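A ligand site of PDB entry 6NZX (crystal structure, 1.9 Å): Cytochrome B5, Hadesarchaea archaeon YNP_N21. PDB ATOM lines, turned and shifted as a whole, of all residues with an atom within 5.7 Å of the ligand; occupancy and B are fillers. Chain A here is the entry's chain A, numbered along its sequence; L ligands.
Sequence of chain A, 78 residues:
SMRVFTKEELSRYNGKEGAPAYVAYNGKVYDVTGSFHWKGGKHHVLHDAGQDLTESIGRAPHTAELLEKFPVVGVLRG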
ATOM      1  N   VAL A  23     -27.240  21.812 -11.483  1.00  0.00           N
ATOM      2  CA  VAL A  23     -26.154  21.136 -10.788  1.00  0.00           C
ATOM      3  C   VAL A  23     -26.756  20.498  -9.542  1.00  0.00           C
ATOM      4  O   VAL A  23     -27.621  21.094  -8.934  1.00  0.00           O
ATOM      5  CB  VAL A  23     -25.018  22.100 -10.405  1.00  0.00           C
ATOM      6  CG1 VAL A  23     -24.311  22.632 -11.642  1.00  0.00           C
ATOM      7  CG2 VAL A  23     -25.513  23.271  -9.552  1.00  0.00           C
ATOM      8  N   ALA A  24     -26.285  19.293  -9.177  1.00  0.00           N
ATOM      9  CA  ALA A  24     -26.779  18.657  -7.959  1.00  0.00           C
ATOM     10  C   ALA A  24     -25.741  18.827  -6.849  1.00  0.00           C
ATOM     11  O   ALA A  24     -24.519  18.915  -7.110  1.00  0.00           O
ATOM     12  CB  ALA A  24     -27.140  17.211  -8.206  1.00  0.00           C
ATOM     13  N   TYR A  25     -26.245  18.965  -5.622  1.00  0.00           N
ATOM     14  CA  TYR A  25     -25.397  19.061  -4.446  1.00  0.00           C
ATOM     15  C   TYR A  25     -26.157  18.444  -3.263  1.00  0.00           C
ATOM     16  O   TYR A  25     -27.200  18.944  -2.908  1.00  0.00           O
ATOM     17  CB  TYR A  25     -24.989  20.505  -4.134  1.00  0.00           C
ATOM     18  CG  TYR A  25     -24.101  20.582  -2.916  1.00  0.00           C
ATOM     19  CD1 TYR A  25     -24.573  21.061  -1.700  1.00  0.00           C
ATOM     20  CD2 TYR A  25     -22.812  20.093  -2.952  1.00  0.00           C
ATOM     21  CE1 TYR A  25     -23.773  21.082  -0.570  1.00  0.00           C
ATOM     22  CE2 TYR A  25     -21.997  20.079  -1.835  1.00  0.00           C
ATOM     23  CZ  TYR A  25     -22.476  20.586  -0.643  1.00  0.00           C
ATOM     24  OH  TYR A  25     -21.667  20.602   0.451  1.00  0.00           O
ATOM     25  N   VAL A  32     -28.949  26.680 -12.164  1.00  0.00           N
ATOM     26  CA  VAL A  32     -27.929  27.705 -12.203  1.00  0.00           C
ATOM     27  C   VAL A  32     -27.882  28.364 -13.597  1.00  0.00           C
ATOM     28  O   VAL A  32     -26.911  29.067 -13.932  1.00  0.00           O
ATOM     29  CB  VAL A  32     -26.560  27.143 -11.767  1.00  0.00           C
ATOM     30  CG1 VAL A  32     -26.540  26.839 -10.279  1.00  0.00           C
ATOM     31  CG2 VAL A  32     -26.120  25.926 -12.558  1.00  0.00           C
ATOM     32  N   SER A  35     -26.710  32.247 -14.175  1.00  0.00           N
ATOM     33  CA  SER A  35     -25.381  32.462 -13.609  1.00  0.00           C
ATOM     34  C   SER A  35     -24.344  32.449 -14.739  1.00  0.00           C
ATOM     35  O   SER A  35     -24.117  31.402 -15.369  1.00  0.00           O
ATOM     36  CB  SER A  35     -25.055  31.416 -12.570  1.00  0.00           C
ATOM     37  OG  SER A  35     -23.701  31.508 -12.143  1.00  0.00           O
ATOM     38  N   PHE A  36     -23.674  33.575 -14.958  1.00  0.00           N
ATOM     39  CA  PHE A  36     -22.628  33.654 -15.976  1.00  0.00           C
ATOM     40  C   PHE A  36     -21.468  32.709 -15.634  1.00  0.00           C
ATOM     41  O   PHE A  36     -20.704  32.336 -16.511  1.00  0.00           O
ATOM     42  CB  PHE A  36     -22.137  35.082 -16.203  1.00  0.00           C
ATOM     43  CG  PHE A  36     -21.417  35.187 -17.516  1.00  0.00           C
ATOM     44  CD1 PHE A  36     -22.137  35.244 -18.704  1.00  0.00           C
ATOM     45  CD2 PHE A  36     -20.028  35.106 -17.573  1.00  0.00           C
ATOM     46  CE1 PHE A  36     -21.470  35.283 -19.929  1.00  0.00           C
ATOM     47  CE2 PHE A  36     -19.369  35.129 -18.797  1.00  0.00           C
ATOM     48  CZ  PHE A  36     -20.095  35.224 -19.968  1.00  0.00           C
ATOM     49  N   HIS A  37     -21.369  32.288 -14.368  1.00  0.00           N
ATOM     50  CA  HIS A  37     -20.391  31.271 -13.955  1.00  0.00           C
ATOM     51  C   HIS A  37     -20.692  29.900 -14.570  1.00  0.00           C
ATOM     52  O   HIS A  37     -19.815  29.058 -14.620  1.00  0.00           O
ATOM     53  CB  HIS A  37     -20.341  31.193 -12.419  1.00  0.00           C
ATOM     54  CG  HIS A  37     -19.868  32.461 -11.815  1.00  0.00           C
ATOM     55  ND1 HIS A  37     -18.536  32.676 -11.475  1.00  0.00           N
ATOM     56  CD2 HIS A  37     -20.515  33.617 -11.544  1.00  0.00           C
ATOM     57  CE1 HIS A  37     -18.398  33.897 -11.004  1.00  0.00           C
ATOM     58  NE2 HIS A  37     -19.598  34.488 -11.010  1.00  0.00           N
ATOM     59  N   TRP A  38     -21.942  29.684 -14.998  1.00  0.00           N
ATOM     60  CA  TRP A  38     -22.372  28.373 -15.488  1.00  0.00           C
ATOM     61  C   TRP A  38     -22.893  28.413 -16.930  1.00  0.00           C
ATOM     62  O   TRP A  38     -23.328  27.373 -17.411  1.00  0.00           O
ATOM     63  CB  TRP A  38     -23.451  27.818 -14.566  1.00  0.00           C
ATOM     64  CG  TRP A  38     -22.889  27.359 -13.257  1.00  0.00           C
ATOM     65  CD1 TRP A  38     -22.795  28.068 -12.103  1.00  0.00           C
ATOM     66  CD2 TRP A  38     -22.292  26.077 -13.003  1.00  0.00           C
ATOM     67  NE1 TRP A  38     -22.231  27.300 -11.124  1.00  0.00           N
ATOM     68  CE2 TRP A  38     -21.898  26.080 -11.648  1.00  0.00           C
ATOM     69  CE3 TRP A  38     -22.092  24.928 -13.770  1.00  0.00           C
ATOM     70  CZ2 TRP A  38     -21.305  24.978 -11.061  1.00  0.00           C
ATOM     71  CZ3 TRP A  38     -21.491  23.842 -13.184  1.00  0.00           C
ATOM     72  CH2 TRP A  38     -21.095  23.875 -11.848  1.00  0.00           C
ATOM     73  N   HIS A  43     -18.125  25.499 -15.663  1.00  0.00           N
ATOM     74  CA  HIS A  43     -17.838  26.286 -14.452  1.00  0.00           C
ATOM     75  C   HIS A  43     -16.318  26.293 -14.230  1.00  0.00           C
ATOM     76  O   HIS A  43     -15.745  25.336 -13.719  1.00  0.00           O
ATOM     77  CB  HIS A  43     -18.638  25.748 -13.255  1.00  0.00           C
ATOM     78  CG  HIS A  43     -18.554  26.584 -12.014  1.00  0.00           C
ATOM     79  ND1 HIS A  43     -18.947  27.909 -11.997  1.00  0.00           N
ATOM     80  CD2 HIS A  43     -18.179  26.278 -10.757  1.00  0.00           C
ATOM     81  CE1 HIS A  43     -18.771  28.389 -10.776  1.00  0.00           C
ATOM     82  NE2 HIS A  43     -18.292  27.409  -9.990  1.00  0.00           N
ATOM     83  N   HIS A  44     -15.674  27.370 -14.702  1.00  0.00           N
ATOM     84  CA  HIS A  44     -14.235  27.649 -14.441  1.00  0.00           C
ATOM     85  C   HIS A  44     -13.374  26.436 -14.801  1.00  0.00           C
ATOM     86  O   HIS A  44     -12.504  26.046 -14.016  1.00  0.00           O
ATOM     87  CB  HIS A  44     -14.039  28.143 -13.001  1.00  0.00           C
ATOM     88  CG  HIS A  44     -14.810  29.396 -12.740  1.00  0.00           C
ATOM     89  ND1 HIS A  44     -14.534  30.583 -13.406  1.00  0.00           N
ATOM     90  CD2 HIS A  44     -15.895  29.632 -11.979  1.00  0.00           C
ATOM     91  CE1 HIS A  44     -15.407  31.510 -13.034  1.00  0.00           C
ATOM     92  NE2 HIS A  44     -16.252  30.949 -12.155  1.00  0.00           N
ATOM     93  N   LEU A  46     -13.042  23.373 -14.765  1.00  0.00           N
ATOM     94  CA  LEU A  46     -12.926  22.082 -14.083  1.00  0.00           C
ATOM     95  C   LEU A  46     -14.272  21.353 -13.993  1.00  0.00           C
ATOM     96  O   LEU A  46     -14.288  20.139 -13.802  1.00  0.00           O
ATOM     97  CB  LEU A  46     -12.368  22.352 -12.690  1.00  0.00           C
ATOM     98  CG  LEU A  46     -10.897  22.756 -12.615  1.00  0.00           C
ATOM     99  CD1 LEU A  46     -10.434  22.792 -11.167  1.00  0.00           C
ATOM    100  CD2 LEU A  46     -10.029  21.779 -13.410  1.00  0.00           C
ATOM    101  N   HIS A  47     -15.400  22.090 -14.097  1.00  0.00           N
ATOM    102  CA  HIS A  47     -16.719  21.597 -13.693  1.00  0.00           C
ATOM    103  C   HIS A  47     -17.731  21.685 -14.849  1.00  0.00           C
ATOM    104  O   HIS A  47     -17.747  22.646 -15.642  1.00  0.00           O
ATOM    105  CB  HIS A  47     -17.214  22.337 -12.432  1.00  0.00           C
ATOM    106  CG  HIS A  47     -16.164  22.473 -11.371  1.00  0.00           C
ATOM    107  ND1 HIS A  47     -15.722  21.392 -10.641  1.00  0.00           N
ATOM    108  CD2 HIS A  47     -15.460  23.540 -10.949  1.00  0.00           C
ATOM    109  CE1 HIS A  47     -14.796  21.777  -9.797  1.00  0.00           C
ATOM    110  NE2 HIS A  47     -14.614  23.121  -9.950  1.00  0.00           N
ATOM    111  N   LEU A  53     -22.039  17.330  -8.141  1.00  0.00           N
ATOM    112  CA  LEU A  53     -20.739  17.864  -7.897  1.00  0.00           C
ATOM    113  C   LEU A  53     -20.496  17.984  -6.384  1.00  0.00           C
ATOM    114  O   LEU A  53     -19.684  18.834  -5.926  1.00  0.00           O
ATOM    115  CB  LEU A  53     -20.646  19.208  -8.624  1.00  0.00           C
ATOM    116  CG  LEU A  53     -20.809  19.162 -10.150  1.00  0.00           C
ATOM    117  CD1 LEU A  53     -20.626  20.544 -10.738  1.00  0.00           C
ATOM    118  CD2 LEU A  53     -19.823  18.190 -10.776  1.00  0.00           C
ATOM    119  N   THR A  54     -21.150  17.117  -5.603  1.00  0.00           N
ATOM    120  CA  THR A  54     -21.052  17.141  -4.162  1.00  0.00           C
ATOM    121  C   THR A  54     -19.575  17.050  -3.747  1.00  0.00           C
ATOM    122  O   THR A  54     -19.086  17.911  -3.015  1.00  0.00           O
ATOM    123  CB  THR A  54     -21.882  16.006  -3.532  1.00  0.00           C
ATOM    124  OG1 THR A  54     -23.248  16.139  -3.893  1.00  0.00           O
ATOM    125  CG2 THR A  54     -21.781  15.973  -2.025  1.00  0.00           C
ATOM    126  N   SER A  56     -16.933  17.555  -5.610  1.00  0.00           N
ATOM    127  CA  SER A  56     -16.139  18.568  -6.332  1.00  0.00           C
ATOM    128  C   SER A  56     -15.961  19.867  -5.540  1.00  0.00           C
ATOM    129  O   SER A  56     -15.115  20.668  -5.885  1.00  0.00           O
ATOM    130  CB  SER A  56     -16.753  18.869  -7.685  1.00  0.00           C
ATOM    131  OG  SER A  56     -16.799  17.695  -8.502  1.00  0.00           O
ATOM    132  N   ILE A  57     -16.793  20.113  -4.517  1.00  0.00           N
ATOM    133  CA  ILE A  57     -16.849  21.436  -3.865  1.00  0.00           C
ATOM    134  C   ILE A  57     -15.576  21.642  -3.014  1.00  0.00           C
ATOM    135  O   ILE A  57     -15.165  22.794  -2.783  1.00  0.00           O
ATOM    136  CB  ILE A  57     -18.136  21.591  -3.034  1.00  0.00           C
ATOM    137  CG1 ILE A  57     -18.458  23.063  -2.720  1.00  0.00           C
ATOM    138  CG2 ILE A  57     -18.070  20.750  -1.762  1.00  0.00           C
ATOM    139  CD1 ILE A  57     -18.867  23.890  -3.930  1.00  0.00           C
ATOM    140  N   ARG A  59     -12.479  21.295  -3.567  1.00  0.00           N
ATOM    141  CA  ARG A  59     -11.381  21.954  -4.270  1.00  0.00           C
ATOM    142  C   ARG A  59     -11.770  23.381  -4.701  1.00  0.00           C
ATOM    143  O   ARG A  59     -10.896  24.153  -5.062  1.00  0.00           O
ATOM    144  CB  ARG A  59     -10.971  21.067  -5.451  1.00  0.00           C
ATOM    145  CG  ARG A  59     -10.536  19.661  -5.051  1.00  0.00           C
ATOM    146  CD  ARG A  59     -10.742  18.598  -6.124  1.00  0.00           C
ATOM    147  NE  ARG A  59      -9.795  17.507  -5.967  1.00  0.00           N
ATOM    148  CZ  ARG A  59      -8.649  17.381  -6.634  1.00  0.00           C
ATOM    149  NH1 ARG A  59      -8.451  18.039  -7.766  1.00  0.00           N
ATOM    150  NH2 ARG A  59      -7.684  16.602  -6.161  1.00  0.00           N
ATOM    151  N   ALA A  60     -13.065  23.737  -4.653  1.00  0.00           N
ATOM    152  CA  ALA A  60     -13.537  25.071  -5.058  1.00  0.00           C
ATOM    153  C   ALA A  60     -12.959  26.136  -4.136  1.00  0.00           C
ATOM    154  O   ALA A  60     -12.727  25.842  -2.966  1.00  0.00           O
ATOM    155  CB  ALA A  60     -15.052  25.117  -5.033  1.00  0.00           C
ATOM    156  N   PRO A  61     -12.813  27.399  -4.598  1.00  0.00           N
ATOM    157  CA  PRO A  61     -12.405  28.524  -3.735  1.00  0.00           C
ATOM    158  C   PRO A  61     -13.578  29.138  -2.952  1.00  0.00           C
ATOM    159  O   PRO A  61     -13.576  30.325  -2.625  1.00  0.00           O
ATOM    160  CB  PRO A  61     -11.892  29.558  -4.748  1.00  0.00           C
ATOM    161  CG  PRO A  61     -12.819  29.351  -5.941  1.00  0.00           C
ATOM    162  CD  PRO A  61     -13.057  27.852  -5.976  1.00  0.00           C
ATOM    163  N   HIS A  62     -14.587  28.314  -2.684  1.00  0.00           N
ATOM    164  CA  HIS A  62     -15.840  28.726  -2.087  1.00  0.00           C
ATOM    165  C   HIS A  62     -16.518  27.484  -1.513  1.00  0.00           C
ATOM    166  O   HIS A  62     -15.983  26.372  -1.661  1.00  0.00           O
ATOM    167  CB  HIS A  62     -16.709  29.461  -3.132  1.00  0.00           C
ATOM    168  CG  HIS A  62     -17.216  28.611  -4.248  1.00  0.00           C
ATOM    169  ND1 HIS A  62     -18.192  27.641  -4.079  1.00  0.00           N
ATOM    170  CD2 HIS A  62     -16.927  28.620  -5.579  1.00  0.00           C
ATOM    171  CE1 HIS A  62     -18.460  27.088  -5.244  1.00  0.00           C
ATOM    172  NE2 HIS A  62     -17.720  27.674  -6.199  1.00  0.00           N
ATOM    173  N   LEU A  66     -23.227  29.249  -1.890  1.00  0.00           N
ATOM    174  CA  LEU A  66     -23.518  30.081  -3.063  1.00  0.00           C
ATOM    175  C   LEU A  66     -24.674  29.483  -3.895  1.00  0.00           C
ATOM    176  O   LEU A  66     -25.311  30.196  -4.644  1.00  0.00           O
ATOM    177  CB  LEU A  66     -22.233  30.234  -3.888  1.00  0.00           C
ATOM    178  CG  LEU A  66     -21.046  30.919  -3.202  1.00  0.00           C
ATOM    179  CD1 LEU A  66     -19.886  31.090  -4.174  1.00  0.00           C
ATOM    180  CD2 LEU A  66     -21.445  32.274  -2.620  1.00  0.00           C
ATOM    181  N   LEU A  67     -24.952  28.182  -3.757  1.00  0.00           N
ATOM    182  CA  LEU A  67     -26.117  27.532  -4.416  1.00  0.00           C
ATOM    183  C   LEU A  67     -27.451  28.119  -3.927  1.00  0.00           C
ATOM    184  O   LEU A  67     -28.485  27.942  -4.584  1.00  0.00           O
ATOM    185  CB  LEU A  67     -26.049  26.031  -4.151  1.00  0.00           C
ATOM    186  CG  LEU A  67     -25.044  25.285  -5.035  1.00  0.00           C
ATOM    187  CD1 LEU A  67     -24.724  23.886  -4.509  1.00  0.00           C
ATOM    188  CD2 LEU A  67     -25.549  25.207  -6.449  1.00  0.00           C
ATOM    189  N   LYS A  69     -28.708  31.074  -3.726  1.00  0.00           N
ATOM    190  CA  LYS A  69     -29.316  32.108  -4.535  1.00  0.00           C
ATOM    191  C   LYS A  69     -30.153  31.512  -5.682  1.00  0.00           C
ATOM    192  O   LYS A  69     -30.934  32.241  -6.301  1.00  0.00           O
ATOM    193  CB  LYS A  69     -28.223  33.045  -5.082  1.00  0.00           C
ATOM    194  CG  LYS A  69     -27.285  33.629  -4.032  1.00  0.00           C
ATOM    195  CD  LYS A  69     -26.328  34.684  -4.535  1.00  0.00           C
ATOM    196  CE  LYS A  69     -25.904  34.493  -5.977  1.00  0.00           C
ATOM    197  NZ  LYS A  69     -24.867  35.486  -6.361  1.00  0.00           N
ATOM    198  N   PHE A  70     -29.998  30.207  -5.963  1.00  0.00           N
ATOM    199  CA  PHE A  70     -30.595  29.570  -7.146  1.00  0.00           C
ATOM    200  C   PHE A  70     -31.789  28.678  -6.758  1.00  0.00           C
ATOM    201  O   PHE A  70     -31.805  28.046  -5.697  1.00  0.00           O
ATOM    202  CB  PHE A  70     -29.491  28.817  -7.885  1.00  0.00           C
ATOM    203  CG  PHE A  70     -28.430  29.766  -8.378  1.00  0.00           C
ATOM    204  CD1 PHE A  70     -28.678  30.553  -9.499  1.00  0.00           C
ATOM    205  CD2 PHE A  70     -27.253  29.949  -7.685  1.00  0.00           C
ATOM    206  CE1 PHE A  70     -27.760  31.488  -9.936  1.00  0.00           C
ATOM    207  CE2 PHE A  70     -26.319  30.882  -8.130  1.00  0.00           C
ATOM    208  CZ  PHE A  70     -26.579  31.649  -9.241  1.00  0.00           C
HETATM  209  C1  LIG L   1     -19.253  30.788  -7.892  1.00  0.00           C
HETATM  210  C2  LIG L   1     -14.852  28.779  -8.891  1.00  0.00           C
HETATM  211  C3  LIG L   1     -16.798  24.340  -8.181  1.00  0.00           C
HETATM  212  C4  LIG L   1     -21.178  26.368  -7.535  1.00  0.00           C
HETATM  213  C5  LIG L   1     -17.835  30.617  -8.177  1.00  0.00           C
HETATM  214  C6  LIG L   1     -16.979  31.797  -8.377  1.00  0.00           C
HETATM  215  C7  LIG L   1     -15.667  31.167  -8.671  1.00  0.00           C
HETATM  216  C8  LIG L   1     -15.906  29.783  -8.610  1.00  0.00           C
HETATM  217  C9  LIG L   1     -14.380  31.904  -8.960  1.00  0.00           C
HETATM  218  C10 LIG L   1     -17.396  33.258  -8.251  1.00  0.00           C
HETATM  219  C11 LIG L   1     -17.474  33.681  -6.765  1.00  0.00           C
HETATM  220  C12 LIG L   1     -18.785  34.368  -6.369  1.00  0.00           C
HETATM  221  O1  LIG L   1     -19.227  34.177  -5.207  1.00  0.00           O
HETATM  222  O2  LIG L   1     -19.390  35.114  -7.173  1.00  0.00           O
HETATM  223  C13 LIG L   1     -14.972  27.313  -8.837  1.00  0.00           C
HETATM  224  C14 LIG L   1     -13.894  26.449  -9.059  1.00  0.00           C
HETATM  225  C15 LIG L   1     -14.450  25.094  -8.832  1.00  0.00           C
HETATM  226  C16 LIG L   1     -15.844  25.406  -8.488  1.00  0.00           C
HETATM  227  C17 LIG L   1     -12.468  26.764  -9.444  1.00  0.00           C
HETATM  228  C18 LIG L   1     -13.875  23.688  -8.976  1.00  0.00           C
HETATM  229  C19 LIG L   1     -12.872  23.315  -7.902  1.00  0.00           C
HETATM  230  C20 LIG L   1     -18.212  24.476  -7.889  1.00  0.00           C
HETATM  231  C21 LIG L   1     -18.990  23.354  -7.687  1.00  0.00           C
HETATM  232  C22 LIG L   1     -20.333  23.923  -7.522  1.00  0.00           C
HETATM  233  C23 LIG L   1     -20.120  25.370  -7.632  1.00  0.00           C
HETATM  234  C24 LIG L   1     -18.465  21.947  -7.695  1.00  0.00           C
HETATM  235  C25 LIG L   1     -21.656  23.310  -7.206  1.00  0.00           C
HETATM  236  C26 LIG L   1     -21.787  22.062  -6.802  1.00  0.00           C
HETATM  237  C27 LIG L   1     -21.054  27.825  -7.592  1.00  0.00           C
HETATM  238  C28 LIG L   1     -22.156  28.658  -7.443  1.00  0.00           C
HETATM  239  C29 LIG L   1     -21.590  30.002  -7.529  1.00  0.00           C
HETATM  240  C30 LIG L   1     -20.233  29.729  -7.736  1.00  0.00           C
HETATM  241  C31 LIG L   1     -23.590  28.276  -7.206  1.00  0.00           C
HETATM  242  C32 LIG L   1     -22.325  31.332  -7.441  1.00  0.00           C
HETATM  243  C33 LIG L   1     -22.773  31.707  -8.857  1.00  0.00           C
HETATM  244  C34 LIG L   1     -23.410  33.076  -8.949  1.00  0.00           C
HETATM  245  O3  LIG L   1     -23.798  33.499 -10.065  1.00  0.00           O
HETATM  246  O4  LIG L   1     -23.545  33.761  -7.922  1.00  0.00           O
HETATM  247  N1  LIG L   1     -17.191  29.447  -8.348  1.00  0.00           N
HETATM  248  N2  LIG L   1     -16.136  26.703  -8.493  1.00  0.00           N
HETATM  249  N3  LIG L   1     -18.829  25.658  -7.881  1.00  0.00           N
HETATM  250  N4  LIG L   1     -19.875  28.441  -7.771  1.00  0.00           N
HETATM  251 FE1  LIG L   1     -18.007  27.545  -8.105  1.00  0.00          FE
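A carbon (C18) of the ligand is covalently linked to a ring nitrogen (NE2) of His 47, at 1.3 Å.
An oxygen (O4) of the ligand is in salt-bridge range of the side-chain amino group (NZ) of Lys 69 (2.7 Å).
NE2 of His 43 is bound to FE1 of the ligand.
The side-chain hydroxyl (OG) of Ser 35 is in hydrogen-bond range of an oxygen (O3) of the ligand (2.9 Å).
NE2 of His 62 is bound to FE1 of the ligand (1.9 Å).
The backbone NH (N) of Leu 53 lies within hydrogen-bond range of the backbone carbonyl oxygen (O) of Ala 24 (3.1 Å).
The side-chain hydroxyl of Ser 35 sits close to the backbone NH of His 37, at 3.3 Å.
A ring nitrogen (ND1) of His 37 is in hydrogen-bond range of a ring nitrogen (NE2) of His 44 (2.9 Å).
ND1 of His 43 lies within hydrogen-bond range of NE1 of Trp 38, 3.5 Å away.
The backbone carbonyl oxygen of His 37 is in hydrogen-bond range of a ring nitrogen (ND1) of His 43.
Merely in contact with the ligand: His 37, Ala 60, Leu 66, His 44, Arg 59, Phe 70, Pro 61, Ser 56, Leu 53, Trp 38, Leu 67 and Ile 57.
Hydrophobic or aromatic side chains that line the ligand: His 37, Trp 38, His 43, His 44, His 47, Leu 53, Ile 57, Ala 60, Pro 61, His 62, Leu 66, Leu 67 and Phe 70.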
